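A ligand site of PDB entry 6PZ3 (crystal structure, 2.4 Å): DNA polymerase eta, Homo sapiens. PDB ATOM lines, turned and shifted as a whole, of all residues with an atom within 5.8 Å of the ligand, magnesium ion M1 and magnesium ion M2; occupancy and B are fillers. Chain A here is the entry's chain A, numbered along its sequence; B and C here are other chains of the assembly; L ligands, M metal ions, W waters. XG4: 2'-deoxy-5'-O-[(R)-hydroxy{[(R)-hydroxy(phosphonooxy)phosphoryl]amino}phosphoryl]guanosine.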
ATOM      1  N   ASP A  16       2.599 -24.888 -15.368  1.00  0.00           N
ATOM      2  CA  ASP A  16       3.037 -25.228 -14.029  1.00  0.00           C
ATOM      3  C   ASP A  16       1.981 -26.096 -13.363  1.00  0.00           C
ATOM      4  O   ASP A  16       0.814 -25.705 -13.280  1.00  0.00           O
ATOM      5  CB  ASP A  16       3.287 -23.969 -13.206  1.00  0.00           C
ATOM      6  CG  ASP A  16       3.923 -24.301 -11.903  1.00  0.00           C
ATOM      7  OD1 ASP A  16       3.198 -24.850 -11.050  1.00  0.00           O
ATOM      8  OD2 ASP A  16       5.160 -24.069 -11.776  1.00  0.00           O
ATOM      9  N   MET A  17       2.399 -27.272 -12.893  1.00  0.00           N
ATOM     10  CA  MET A  17       1.478 -28.180 -12.245  1.00  0.00           C
ATOM     11  C   MET A  17       1.035 -27.588 -10.908  1.00  0.00           C
ATOM     12  O   MET A  17       1.860 -27.140 -10.120  1.00  0.00           O
ATOM     13  CB  MET A  17       2.120 -29.551 -12.023  1.00  0.00           C
ATOM     14  CG  MET A  17       2.724 -30.194 -13.278  1.00  0.00           C
ATOM     15  SD  MET A  17       1.622 -30.174 -14.708  1.00  0.00           S
ATOM     16  CE  MET A  17       0.258 -31.155 -14.096  1.00  0.00           C
ATOM     17  N   ASP A  18      -0.274 -27.600 -10.664  1.00  0.00           N
ATOM     18  CA  ASP A  18      -0.812 -27.101  -9.402  1.00  0.00           C
ATOM     19  C   ASP A  18      -0.433 -28.044  -8.265  1.00  0.00           C
ATOM     20  O   ASP A  18      -0.642 -29.263  -8.365  1.00  0.00           O
ATOM     21  CB  ASP A  18      -2.332 -26.946  -9.505  1.00  0.00           C
ATOM     22  CG  ASP A  18      -2.755 -25.995 -10.620  1.00  0.00           C
ATOM     23  OD1 ASP A  18      -2.006 -25.048 -10.921  1.00  0.00           O
ATOM     24  OD2 ASP A  18      -3.850 -26.191 -11.192  1.00  0.00           O
ATOM     25  N   CYS A  19       0.112 -27.473  -7.178  1.00  0.00           N
ATOM     26  CA  CYS A  19       0.551 -28.210  -5.988  1.00  0.00           C
ATOM     27  C   CYS A  19       0.990 -29.629  -6.356  1.00  0.00           C
ATOM     28  O   CYS A  19       0.362 -30.611  -5.939  1.00  0.00           O
ATOM     29  CB  CYS A  19      -0.545 -28.226  -4.912  1.00  0.00           C
ATOM     30  SG  CYS A  19      -2.188 -28.618  -5.493  1.00  0.00           S
ATOM     31  N   PHE A  20       2.086 -29.737  -7.113  1.00  0.00           N
ATOM     32  CA  PHE A  20       2.338 -30.935  -7.897  1.00  0.00           C
ATOM     33  C   PHE A  20       2.482 -32.173  -7.025  1.00  0.00           C
ATOM     34  O   PHE A  20       1.811 -33.180  -7.238  1.00  0.00           O
ATOM     35  CB  PHE A  20       3.598 -30.750  -8.750  1.00  0.00           C
ATOM     36  CG  PHE A  20       3.919 -31.935  -9.620  1.00  0.00           C
ATOM     37  CD1 PHE A  20       2.933 -32.546 -10.375  1.00  0.00           C
ATOM     38  CD2 PHE A  20       5.199 -32.436  -9.677  1.00  0.00           C
ATOM     39  CE1 PHE A  20       3.223 -33.632 -11.166  1.00  0.00           C
ATOM     40  CE2 PHE A  20       5.493 -33.528 -10.476  1.00  0.00           C
ATOM     41  CZ  PHE A  20       4.508 -34.126 -11.212  1.00  0.00           C
ATOM     42  N   PHE A  21       3.385 -32.124  -6.033  1.00  0.00           N
ATOM     43  CA  PHE A  21       3.600 -33.307  -5.206  1.00  0.00           C
ATOM     44  C   PHE A  21       2.306 -33.731  -4.513  1.00  0.00           C
ATOM     45  O   PHE A  21       2.063 -34.929  -4.360  1.00  0.00           O
ATOM     46  CB  PHE A  21       4.702 -33.051  -4.175  1.00  0.00           C
ATOM     47  CG  PHE A  21       6.084 -32.983  -4.747  1.00  0.00           C
ATOM     48  CD1 PHE A  21       6.302 -32.788  -6.098  1.00  0.00           C
ATOM     49  CD2 PHE A  21       7.194 -33.097  -3.917  1.00  0.00           C
ATOM     50  CE1 PHE A  21       7.585 -32.711  -6.616  1.00  0.00           C
ATOM     51  CE2 PHE A  21       8.473 -33.024  -4.421  1.00  0.00           C
ATOM     52  CZ  PHE A  21       8.659 -32.826  -5.779  1.00  0.00           C
ATOM     53  N   VAL A  22       1.456 -32.763  -4.132  1.00  0.00           N
ATOM     54  CA  VAL A  22       0.156 -33.087  -3.542  1.00  0.00           C
ATOM     55  C   VAL A  22      -0.702 -33.832  -4.558  1.00  0.00           C
ATOM     56  O   VAL A  22      -1.276 -34.890  -4.248  1.00  0.00           O
ATOM     57  CB  VAL A  22      -0.532 -31.801  -3.041  1.00  0.00           C
ATOM     58  CG1 VAL A  22      -1.981 -32.030  -2.758  1.00  0.00           C
ATOM     59  CG2 VAL A  22       0.146 -31.297  -1.800  1.00  0.00           C
ATOM     60  N   GLN A  41       8.411 -34.144   4.314  1.00  0.00           N
ATOM     61  CA  GLN A  41       9.561 -35.041   4.407  1.00  0.00           C
ATOM     62  C   GLN A  41      10.182 -34.980   5.803  1.00  0.00           C
ATOM     63  O   GLN A  41      10.438 -33.909   6.353  1.00  0.00           O
ATOM     64  CB  GLN A  41      10.624 -34.757   3.320  1.00  0.00           C
ATOM     65  CG  GLN A  41      11.083 -33.349   3.046  1.00  0.00           C
ATOM     66  CD  GLN A  41      12.032 -33.264   1.821  1.00  0.00           C
ATOM     67  OE1 GLN A  41      11.978 -34.094   0.916  1.00  0.00           O
ATOM     68  NE2 GLN A  41      12.917 -32.284   1.820  1.00  0.00           N
ATOM     69  N   ILE A  51       6.769 -29.330   1.929  1.00  0.00           N
ATOM     70  CA  ILE A  51       7.295 -28.936   0.631  1.00  0.00           C
ATOM     71  C   ILE A  51       6.211 -28.727  -0.423  1.00  0.00           C
ATOM     72  O   ILE A  51       6.533 -28.239  -1.516  1.00  0.00           O
ATOM     73  CB  ILE A  51       8.339 -29.935   0.106  1.00  0.00           C
ATOM     74  CG1 ILE A  51       7.756 -31.335  -0.042  1.00  0.00           C
ATOM     75  CG2 ILE A  51       9.534 -29.971   1.028  1.00  0.00           C
ATOM     76  CD1 ILE A  51       8.665 -32.264  -0.789  1.00  0.00           C
ATOM     77  N   ALA A  52       4.962 -29.083  -0.158  1.00  0.00           N
ATOM     78  CA  ALA A  52       3.883 -28.848  -1.122  1.00  0.00           C
ATOM     79  C   ALA A  52       2.560 -28.818  -0.368  1.00  0.00           C
ATOM     80  O   ALA A  52       2.357 -29.594   0.564  1.00  0.00           O
ATOM     81  CB  ALA A  52       3.877 -29.940  -2.205  1.00  0.00           C
ATOM     82  N   VAL A  53       1.670 -27.916  -0.784  1.00  0.00           N
ATOM     83  CA  VAL A  53       0.463 -27.583  -0.029  1.00  0.00           C
ATOM     84  C   VAL A  53      -0.715 -27.471  -0.988  1.00  0.00           C
ATOM     85  O   VAL A  53      -0.694 -26.631  -1.891  1.00  0.00           O
ATOM     86  CB  VAL A  53       0.626 -26.261   0.745  1.00  0.00           C
ATOM     87  CG1 VAL A  53      -0.501 -26.064   1.729  1.00  0.00           C
ATOM     88  CG2 VAL A  53       1.963 -26.199   1.455  1.00  0.00           C
ATOM     89  N   TYR A  55      -4.438 -26.337  -2.287  1.00  0.00           N
ATOM     90  CA  TYR A  55      -5.063 -25.008  -2.202  1.00  0.00           C
ATOM     91  C   TYR A  55      -6.079 -24.927  -1.075  1.00  0.00           C
ATOM     92  O   TYR A  55      -6.222 -23.872  -0.454  1.00  0.00           O
ATOM     93  CB  TYR A  55      -5.693 -24.650  -3.556  1.00  0.00           C
ATOM     94  CG  TYR A  55      -4.633 -24.153  -4.514  1.00  0.00           C
ATOM     95  CD1 TYR A  55      -3.817 -25.048  -5.189  1.00  0.00           C
ATOM     96  CD2 TYR A  55      -4.418 -22.798  -4.699  1.00  0.00           C
ATOM     97  CE1 TYR A  55      -2.828 -24.601  -6.041  1.00  0.00           C
ATOM     98  CE2 TYR A  55      -3.426 -22.335  -5.545  1.00  0.00           C
ATOM     99  CZ  TYR A  55      -2.630 -23.240  -6.213  1.00  0.00           C
ATOM    100  OH  TYR A  55      -1.647 -22.780  -7.062  1.00  0.00           O
ATOM    101  N   ARG A  58      -3.857 -24.041   1.719  1.00  0.00           N
ATOM    102  CA  ARG A  58      -3.386 -22.661   1.649  1.00  0.00           C
ATOM    103  C   ARG A  58      -4.401 -21.688   2.219  1.00  0.00           C
ATOM    104  O   ARG A  58      -4.029 -20.706   2.861  1.00  0.00           O
ATOM    105  CB  ARG A  58      -3.054 -22.306   0.201  1.00  0.00           C
ATOM    106  CG  ARG A  58      -1.866 -23.058  -0.339  1.00  0.00           C
ATOM    107  CD  ARG A  58      -1.598 -22.750  -1.807  1.00  0.00           C
ATOM    108  NE  ARG A  58      -0.727 -23.758  -2.411  1.00  0.00           N
ATOM    109  CZ  ARG A  58      -0.125 -23.633  -3.583  1.00  0.00           C
ATOM    110  NH1 ARG A  58      -0.295 -22.532  -4.310  1.00  0.00           N
ATOM    111  NH2 ARG A  58       0.660 -24.602  -4.038  1.00  0.00           N
ATOM    112  N   ARG A  64       4.601 -23.758   2.208  1.00  0.00           N
ATOM    113  CA  ARG A  64       5.856 -24.461   2.025  1.00  0.00           C
ATOM    114  C   ARG A  64       6.895 -23.918   3.005  1.00  0.00           C
ATOM    115  O   ARG A  64       6.864 -22.751   3.389  1.00  0.00           O
ATOM    116  CB  ARG A  64       6.292 -24.277   0.570  1.00  0.00           C
ATOM    117  CG  ARG A  64       7.696 -24.639   0.240  1.00  0.00           C
ATOM    118  CD  ARG A  64       7.963 -24.291  -1.239  1.00  0.00           C
ATOM    119  NE  ARG A  64       7.408 -25.295  -2.152  1.00  0.00           N
ATOM    120  CZ  ARG A  64       6.216 -25.207  -2.768  1.00  0.00           C
ATOM    121  NH1 ARG A  64       5.426 -24.163  -2.593  1.00  0.00           N
ATOM    122  NH2 ARG A  64       5.836 -26.173  -3.579  1.00  0.00           N
ATOM    123  N   SER A 116      11.683 -26.939 -14.271  1.00  0.00           N
ATOM    124  CA  SER A 116      11.817 -27.564 -12.970  1.00  0.00           C
ATOM    125  C   SER A 116      11.068 -28.897 -13.032  1.00  0.00           C
ATOM    126  O   SER A 116      10.557 -29.293 -14.088  1.00  0.00           O
ATOM    127  CB  SER A 116      11.264 -26.671 -11.862  1.00  0.00           C
ATOM    128  OG  SER A 116       9.852 -26.666 -11.905  1.00  0.00           O
ATOM    129  N   ILE A 117      10.968 -29.569 -11.885  1.00  0.00           N
ATOM    130  CA  ILE A 117      10.307 -30.865 -11.881  1.00  0.00           C
ATOM    131  C   ILE A 117       8.851 -30.756 -12.296  1.00  0.00           C
ATOM    132  O   ILE A 117       8.283 -31.732 -12.792  1.00  0.00           O
ATOM    133  CB  ILE A 117      10.426 -31.528 -10.489  1.00  0.00           C
ATOM    134  CG1 ILE A 117      10.080 -33.015 -10.570  1.00  0.00           C
ATOM    135  CG2 ILE A 117       9.544 -30.804  -9.476  1.00  0.00           C
ATOM    136  CD1 ILE A 117      10.369 -33.754  -9.295  1.00  0.00           C
ATOM    137  N   ASP A 118       8.236 -29.579 -12.166  1.00  0.00           N
ATOM    138  CA  ASP A 118       6.803 -29.470 -12.374  1.00  0.00           C
ATOM    139  C   ASP A 118       6.385 -28.368 -13.343  1.00  0.00           C
ATOM    140  O   ASP A 118       5.196 -28.057 -13.406  1.00  0.00           O
ATOM    141  CB  ASP A 118       6.102 -29.251 -11.036  1.00  0.00           C
ATOM    142  CG  ASP A 118       5.835 -27.799 -10.786  1.00  0.00           C
ATOM    143  OD1 ASP A 118       4.646 -27.403 -10.744  1.00  0.00           O
ATOM    144  OD2 ASP A 118       6.831 -27.054 -10.675  1.00  0.00           O
ATOM    145  N   GLU A 119       7.309 -27.778 -14.096  1.00  0.00           N
ATOM    146  CA  GLU A 119       6.920 -26.807 -15.101  1.00  0.00           C
ATOM    147  C   GLU A 119       7.873 -26.852 -16.285  1.00  0.00           C
ATOM    148  O   GLU A 119       9.036 -27.254 -16.170  1.00  0.00           O
ATOM    149  CB  GLU A 119       6.867 -25.380 -14.548  1.00  0.00           C
ATOM    150  CG  GLU A 119       8.154 -24.871 -13.978  1.00  0.00           C
ATOM    151  CD  GLU A 119       7.928 -23.791 -12.927  1.00  0.00           C
ATOM    152  OE1 GLU A 119       8.111 -22.591 -13.206  1.00  0.00           O
ATOM    153  OE2 GLU A 119       7.550 -24.160 -11.807  1.00  0.00           O
ATOM    154  N   LYS A 227       5.680 -16.830 -17.476  1.00  0.00           N
ATOM    155  CA  LYS A 227       5.713 -17.273 -16.082  1.00  0.00           C
ATOM    156  C   LYS A 227       4.930 -16.338 -15.178  1.00  0.00           C
ATOM    157  O   LYS A 227       4.245 -16.787 -14.260  1.00  0.00           O
ATOM    158  CB  LYS A 227       7.158 -17.371 -15.577  1.00  0.00           C
ATOM    159  CG  LYS A 227       7.211 -18.021 -14.203  1.00  0.00           C
ATOM    160  CD  LYS A 227       8.550 -17.927 -13.536  1.00  0.00           C
ATOM    161  CE  LYS A 227       8.497 -18.580 -12.142  1.00  0.00           C
ATOM    162  NZ  LYS A 227       7.883 -19.967 -12.174  1.00  0.00           N
ATOM    163  N   LYS A 234      -4.214 -18.805 -10.600  1.00  0.00           N
ATOM    164  CA  LYS A 234      -4.098 -20.192 -10.185  1.00  0.00           C
ATOM    165  C   LYS A 234      -5.195 -20.516  -9.183  1.00  0.00           C
ATOM    166  O   LYS A 234      -5.623 -19.649  -8.429  1.00  0.00           O
ATOM    167  CB  LYS A 234      -2.728 -20.461  -9.555  1.00  0.00           C
ATOM    168  CG  LYS A 234      -1.690 -21.012 -10.532  1.00  0.00           C
ATOM    169  CD  LYS A 234      -0.283 -21.084  -9.909  1.00  0.00           C
ATOM    170  CE  LYS A 234       0.659 -21.968 -10.741  1.00  0.00           C
ATOM    171  NZ  LYS A 234       0.366 -23.463 -10.633  1.00  0.00           N
ATOM    172  N   PRO A 235      -5.681 -21.767  -9.121  1.00  0.00           N
ATOM    173  CA  PRO A 235      -5.267 -22.956  -9.859  1.00  0.00           C
ATOM    174  C   PRO A 235      -6.159 -23.306 -11.040  1.00  0.00           C
ATOM    175  O   PRO A 235      -7.268 -22.799 -11.175  1.00  0.00           O
ATOM    176  CB  PRO A 235      -5.356 -24.049  -8.791  1.00  0.00           C
ATOM    177  CG  PRO A 235      -6.568 -23.637  -8.009  1.00  0.00           C
ATOM    178  CD  PRO A 235      -6.583 -22.133  -8.012  1.00  0.00           C
ATOM    179  P    DT B   8      10.018 -20.114  -8.529  1.00  0.00           P
ATOM    180  OP1  DT B   8       8.794 -19.744  -9.279  1.00  0.00           O
ATOM    181  OP2  DT B   8      10.180 -19.706  -7.105  1.00  0.00           O
ATOM    182  O5'  DT B   8      10.186 -21.713  -8.540  1.00  0.00           O
ATOM    183  C5'  DT B   8      10.274 -22.422  -9.785  1.00  0.00           C
ATOM    184  C4'  DT B   8      10.304 -23.926  -9.554  1.00  0.00           C
ATOM    185  O4'  DT B   8      11.455 -24.264  -8.722  1.00  0.00           O
ATOM    186  C3'  DT B   8       9.075 -24.460  -8.825  1.00  0.00           C
ATOM    187  O3'  DT B   8       8.625 -25.690  -9.414  1.00  0.00           O
ATOM    188  C2'  DT B   8       9.572 -24.655  -7.396  1.00  0.00           C
ATOM    189  C1'  DT B   8      11.023 -25.010  -7.601  1.00  0.00           C
ATOM    190  N1   DT B   8      11.904 -24.687  -6.422  1.00  0.00           N
ATOM    191  C2   DT B   8      12.592 -25.696  -5.810  1.00  0.00           C
ATOM    192  O2   DT B   8      12.538 -26.856  -6.181  1.00  0.00           O
ATOM    193  N3   DT B   8      13.365 -25.307  -4.757  1.00  0.00           N
ATOM    194  C4   DT B   8      13.515 -24.040  -4.255  1.00  0.00           C
ATOM    195  O4   DT B   8      14.250 -23.794  -3.293  1.00  0.00           O
ATOM    196  C5   DT B   8      12.754 -23.012  -4.945  1.00  0.00           C
ATOM    197  C7   DT B   8      12.810 -21.584  -4.488  1.00  0.00           C
ATOM    198  C6   DT B   8      11.990 -23.385  -5.977  1.00  0.00           C
ATOM    199  P    DT C   3      15.673 -23.710  10.010  1.00  0.00           P
ATOM    200  OP1  DT C   3      16.193 -22.559  10.789  1.00  0.00           O
ATOM    201  OP2  DT C   3      14.270 -23.716   9.539  1.00  0.00           O
ATOM    202  O5'  DT C   3      16.620 -23.946   8.730  1.00  0.00           O
ATOM    203  C5'  DT C   3      16.076 -24.463   7.507  1.00  0.00           C
ATOM    204  C4'  DT C   3      15.392 -25.798   7.728  1.00  0.00           C
ATOM    205  O4'  DT C   3      14.097 -25.795   7.119  1.00  0.00           O
ATOM    206  C3'  DT C   3      16.056 -27.003   7.101  1.00  0.00           C
ATOM    207  O3'  DT C   3      17.182 -27.464   7.850  1.00  0.00           O
ATOM    208  C2'  DT C   3      14.904 -28.016   7.100  1.00  0.00           C
ATOM    209  C1'  DT C   3      13.655 -27.138   7.092  1.00  0.00           C
ATOM    210  N1   DT C   3      12.797 -27.380   5.917  1.00  0.00           N
ATOM    211  C2   DT C   3      12.157 -28.586   5.815  1.00  0.00           C
ATOM    212  O2   DT C   3      12.264 -29.467   6.646  1.00  0.00           O
ATOM    213  N3   DT C   3      11.385 -28.731   4.707  1.00  0.00           N
ATOM    214  C4   DT C   3      11.187 -27.802   3.719  1.00  0.00           C
ATOM    215  O4   DT C   3      10.458 -28.016   2.768  1.00  0.00           O
ATOM    216  C5   DT C   3      11.886 -26.562   3.873  1.00  0.00           C
ATOM    217  C7   DT C   3      11.733 -25.491   2.851  1.00  0.00           C
ATOM    218  C6   DT C   3      12.646 -26.397   4.961  1.00  0.00           C
ATOM    219  P   CAR C   4      18.393 -28.219   7.105  1.00  0.00           P
ATOM    220  OP1 CAR C   4      19.048 -29.183   8.073  1.00  0.00           O
ATOM    221  OP2 CAR C   4      19.243 -27.179   6.416  1.00  0.00           O
ATOM    222  O5' CAR C   4      17.677 -29.113   5.998  1.00  0.00           O
ATOM    223  C5' CAR C   4      16.958 -30.298   6.356  1.00  0.00           C
ATOM    224  C4' CAR C   4      16.221 -30.877   5.179  1.00  0.00           C
ATOM    225  O4' CAR C   4      15.307 -29.907   4.618  1.00  0.00           O
ATOM    226  C3' CAR C   4      17.151 -31.301   4.039  1.00  0.00           C
ATOM    227  O3' CAR C   4      16.836 -32.606   3.609  1.00  0.00           O
ATOM    228  C2' CAR C   4      16.819 -30.337   2.903  1.00  0.00           C
ATOM    229  O2' CAR C   4      17.660 -29.196   2.808  1.00  0.00           O
ATOM    230  C1' CAR C   4      15.379 -29.956   3.215  1.00  0.00           C
ATOM    231  N1  CAR C   4      15.011 -28.669   2.628  1.00  0.00           N
ATOM    232  C2  CAR C   4      14.459 -28.700   1.330  1.00  0.00           C
ATOM    233  O2  CAR C   4      14.259 -29.792   0.772  1.00  0.00           O
ATOM    234  N3  CAR C   4      14.135 -27.573   0.695  1.00  0.00           N
ATOM    235  C4  CAR C   4      14.358 -26.388   1.275  1.00  0.00           C
ATOM    236  N4  CAR C   4      14.002 -25.283   0.597  1.00  0.00           N
ATOM    237  C5  CAR C   4      14.919 -26.325   2.546  1.00  0.00           C
ATOM    238  C6  CAR C   4      15.259 -27.498   3.217  1.00  0.00           C
ATOM    239  P    DA C   5      17.909 -33.394   2.742  1.00  0.00           P
ATOM    240  OP1  DA C   5      17.846 -34.786   3.228  1.00  0.00           O
ATOM    241  OP2  DA C   5      19.181 -32.651   2.802  1.00  0.00           O
ATOM    242  O5'  DA C   5      17.363 -33.271   1.239  1.00  0.00           O
ATOM    243  C5'  DA C   5      16.204 -34.008   0.824  1.00  0.00           C
ATOM    244  C4'  DA C   5      15.942 -33.824  -0.660  1.00  0.00           C
ATOM    245  O4'  DA C   5      15.530 -32.460  -0.929  1.00  0.00           O
ATOM    246  C3'  DA C   5      17.153 -34.075  -1.564  1.00  0.00           C
ATOM    247  O3'  DA C   5      16.751 -34.793  -2.703  1.00  0.00           O
ATOM    248  C2'  DA C   5      17.630 -32.666  -1.893  1.00  0.00           C
ATOM    249  C1'  DA C   5      16.317 -31.915  -1.964  1.00  0.00           C
ATOM    250  N9   DA C   5      16.434 -30.478  -1.776  1.00  0.00           N
ATOM    251  C8   DA C   5      17.204 -29.826  -0.856  1.00  0.00           C
ATOM    252  N7   DA C   5      17.084 -28.524  -0.913  1.00  0.00           N
ATOM    253  C5   DA C   5      16.169 -28.302  -1.918  1.00  0.00           C
ATOM    254  C6   DA C   5      15.613 -27.135  -2.474  1.00  0.00           C
ATOM    255  N6   DA C   5      15.921 -25.907  -2.066  1.00  0.00           N
ATOM    256  N1   DA C   5      14.732 -27.281  -3.486  1.00  0.00           N
ATOM    257  C2   DA C   5      14.429 -28.513  -3.902  1.00  0.00           C
ATOM    258  N3   DA C   5      14.875 -29.679  -3.460  1.00  0.00           N
ATOM    259  C4   DA C   5      15.752 -29.509  -2.464  1.00  0.00           C
HETATM  260  N1  XG4 L   1      11.663 -27.560  -1.340  1.00  0.00           N
HETATM  261  C2  XG4 L   1      11.345 -28.796  -1.775  1.00  0.00           C
HETATM  262  N2  XG4 L   1      11.893 -29.889  -1.216  1.00  0.00           N
HETATM  263  N3  XG4 L   1      10.482 -29.021  -2.782  1.00  0.00           N
HETATM  264  C4  XG4 L   1       9.889 -27.983  -3.410  1.00  0.00           C
HETATM  265  C5  XG4 L   1      10.187 -26.607  -2.980  1.00  0.00           C
HETATM  266  C6  XG4 L   1      11.142 -26.444  -1.872  1.00  0.00           C
HETATM  267  O6  XG4 L   1      11.445 -25.298  -1.457  1.00  0.00           O
HETATM  268  N7  XG4 L   1       9.468 -25.802  -3.772  1.00  0.00           N
HETATM  269  C8  XG4 L   1       8.769 -26.597  -4.632  1.00  0.00           C
HETATM  270  N9  XG4 L   1       9.030 -27.910  -4.412  1.00  0.00           N
HETATM  271  PA  XG4 L   1       6.022 -25.174  -7.276  1.00  0.00           P
HETATM  272  PB  XG4 L   1       3.382 -26.355  -6.469  1.00  0.00           P
HETATM  273  PG  XG4 L   1       1.687 -24.260  -7.325  1.00  0.00           P
HETATM  274  C1' XG4 L   1       8.462 -29.088  -5.112  1.00  0.00           C
HETATM  275  O1A XG4 L   1       5.447 -25.053  -8.651  1.00  0.00           O
HETATM  276  O1B XG4 L   1       3.501 -26.971  -7.818  1.00  0.00           O
HETATM  277  O1G XG4 L   1       2.604 -24.438  -8.515  1.00  0.00           O
HETATM  278  C2' XG4 L   1       7.082 -29.356  -4.547  1.00  0.00           C
HETATM  279  O2A XG4 L   1       6.897 -23.876  -6.903  1.00  0.00           O
HETATM  280  O2B XG4 L   1       3.414 -27.559  -5.397  1.00  0.00           O
HETATM  281  O2G XG4 L   1       0.227 -24.471  -7.653  1.00  0.00           O
HETATM  282  C3' XG4 L   1       6.125 -28.884  -5.622  1.00  0.00           C
HETATM  283  O3' XG4 L   1       4.974 -29.719  -5.702  1.00  0.00           O
HETATM  284  N3A XG4 L   1       4.698 -25.252  -6.147  1.00  0.00           N
HETATM  285  O3B XG4 L   1       2.021 -25.489  -6.326  1.00  0.00           O
HETATM  286  O3G XG4 L   1       1.966 -23.059  -6.452  1.00  0.00           O
HETATM  287  C4' XG4 L   1       6.950 -28.901  -6.895  1.00  0.00           C
HETATM  288  O4' XG4 L   1       8.315 -28.812  -6.508  1.00  0.00           O
HETATM  289  C5' XG4 L   1       6.616 -27.739  -7.814  1.00  0.00           C
HETATM  290  O5' XG4 L   1       6.907 -26.516  -7.142  1.00  0.00           O
HETATM  291 MG    MG M   1       3.729 -25.884  -9.477  1.00  0.00          MG
HETATM  292 MG    MG M   2       6.507 -24.950 -10.445  1.00  0.00          MG
HETATM  293  O   HOH W   1       6.451 -22.932  -9.835  1.00  0.00           O
HETATM  294  O   HOH W   2      12.674 -32.814  -1.449  1.00  0.00           O
HETATM  295  O   HOH W   3       2.716 -26.133  -2.931  1.00  0.00           O
HETATM  296  O   HOH W   4       3.929 -22.508  -4.598  1.00  0.00           O
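Of the 25 residues printed, 4 come within 4 Å of magnesium ion M2. The nearest printed residue that does not touch magnesium ion M2 is Ser 116 (4.03 Å).
The side-chain carboxylate of Glu 119 lies close to the side-chain hydroxyl of Ser 116, at 3.4 Å. The side-chain carboxylate of Glu 119 is in salt-bridge range of the side-chain amino group of Lys 227 (2.8 Å). NZ of Lys 234 lies within hydrogen-bond range of O of Asp 16, 3.5 Å away. The backbone NH (N) of Asp 118 lies close to the side-chain hydroxyl (OG) of Ser 116 (3.3 Å). O3' of DT 8 of chain B sits close to the side-chain hydroxyl (OG) of Ser 116 (2.9 Å). The side-chain amino group (NZ) of Lys 227 is in salt-bridge range of OP1 of DT 8 of chain B (3.0 Å). NE of Arg 58 is in hydrogen-bond range of O of Val 53 (2.9 Å). O2 of CAR 4 of chain C sits at hydrogen-bond distance from NE2 of Gln 41, 3.0 Å away.
The side-chain hydroxyl of Tyr 55 is in hydrogen-bond range of an oxygen (O2G) of the ligand, at 2.6 Å. NH2 of Arg 64 is in salt-bridge range of O2B of the ligand. NH2 of Arg 58 is in salt-bridge range of O3G of the ligand. The backbone NH of Cys 19 sits at hydrogen-bond distance from an oxygen (O3B) of the ligand (2.9 Å). The backbone NH of Phe 21 sits at hydrogen-bond distance from an oxygen (O3') of the ligand (2.9 Å). The backbone NH of Phe 20 sits at hydrogen-bond distance from an oxygen (O2B) of the ligand. O2 of CAR 4 of chain C sits at hydrogen-bond distance from a nitrogen (N2) of the ligand (3.1 Å). The side-chain amino group (NZ) of Lys 234 is in salt-bridge range of an oxygen (O2G) of the ligand (3.1 Å).
Water W4 bridges O3G of the ligand (2.8 Å) and NH1 of Arg 64 (3.0 Å). Water W2 lies within hydrogen-bond range of OE1 of Gln 41 (2.8 Å), O4' of DA 5 of chain C (2.9 Å) and N2 of the ligand (3.0 Å).
Asp 18 touches the ligand. Ile 51 touches the ligand. Ala 52 touches the ligand. Ile 117 touches the ligand (CG2 to O4', 3.8 Å). DA 5 of chain C touches the ligand. Hydrophobic or aromatic side chains that line the ligand: Phe 20, Phe 21, Ile 51, Ala 52, Tyr 55 and Ile 117. 18 residues have an atom within 4 Å of the ligand: Asp 16, Met 17, Asp 18, Cys 19, Phe 20, Phe 21, Ile 51, Ala 52, Tyr 55, Arg 58, Arg 64, Ile 117, Asp 118, Glu 119, Lys 234, DT 8 of chain B, CAR 4 of chain C and DA 5 of chain C.
Magnesium ion M1 is bound by the side-chain carboxylate of Asp 16, an oxygen (O1B) of the ligand, an oxygen (O1G) of the ligand, an oxygen (O1A) of the ligand, the side-chain carboxylate of Asp 118 and the backbone carbonyl oxygen of Met 17.
Magnesium ion M2 is bound by OE2 of Glu 119 (1.9 Å), O1A of the ligand (2.1 Å), OD2 of Asp 16 (2.1 Å), water W1 (2.1 Å), OD2 of Asp 118 (2.1 Å) and O3' of DT 8 of chain B (2.5 Å).
The nearest printed residue that does not touch magnesium ion M1 is Lys 234 (4.3 Å).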
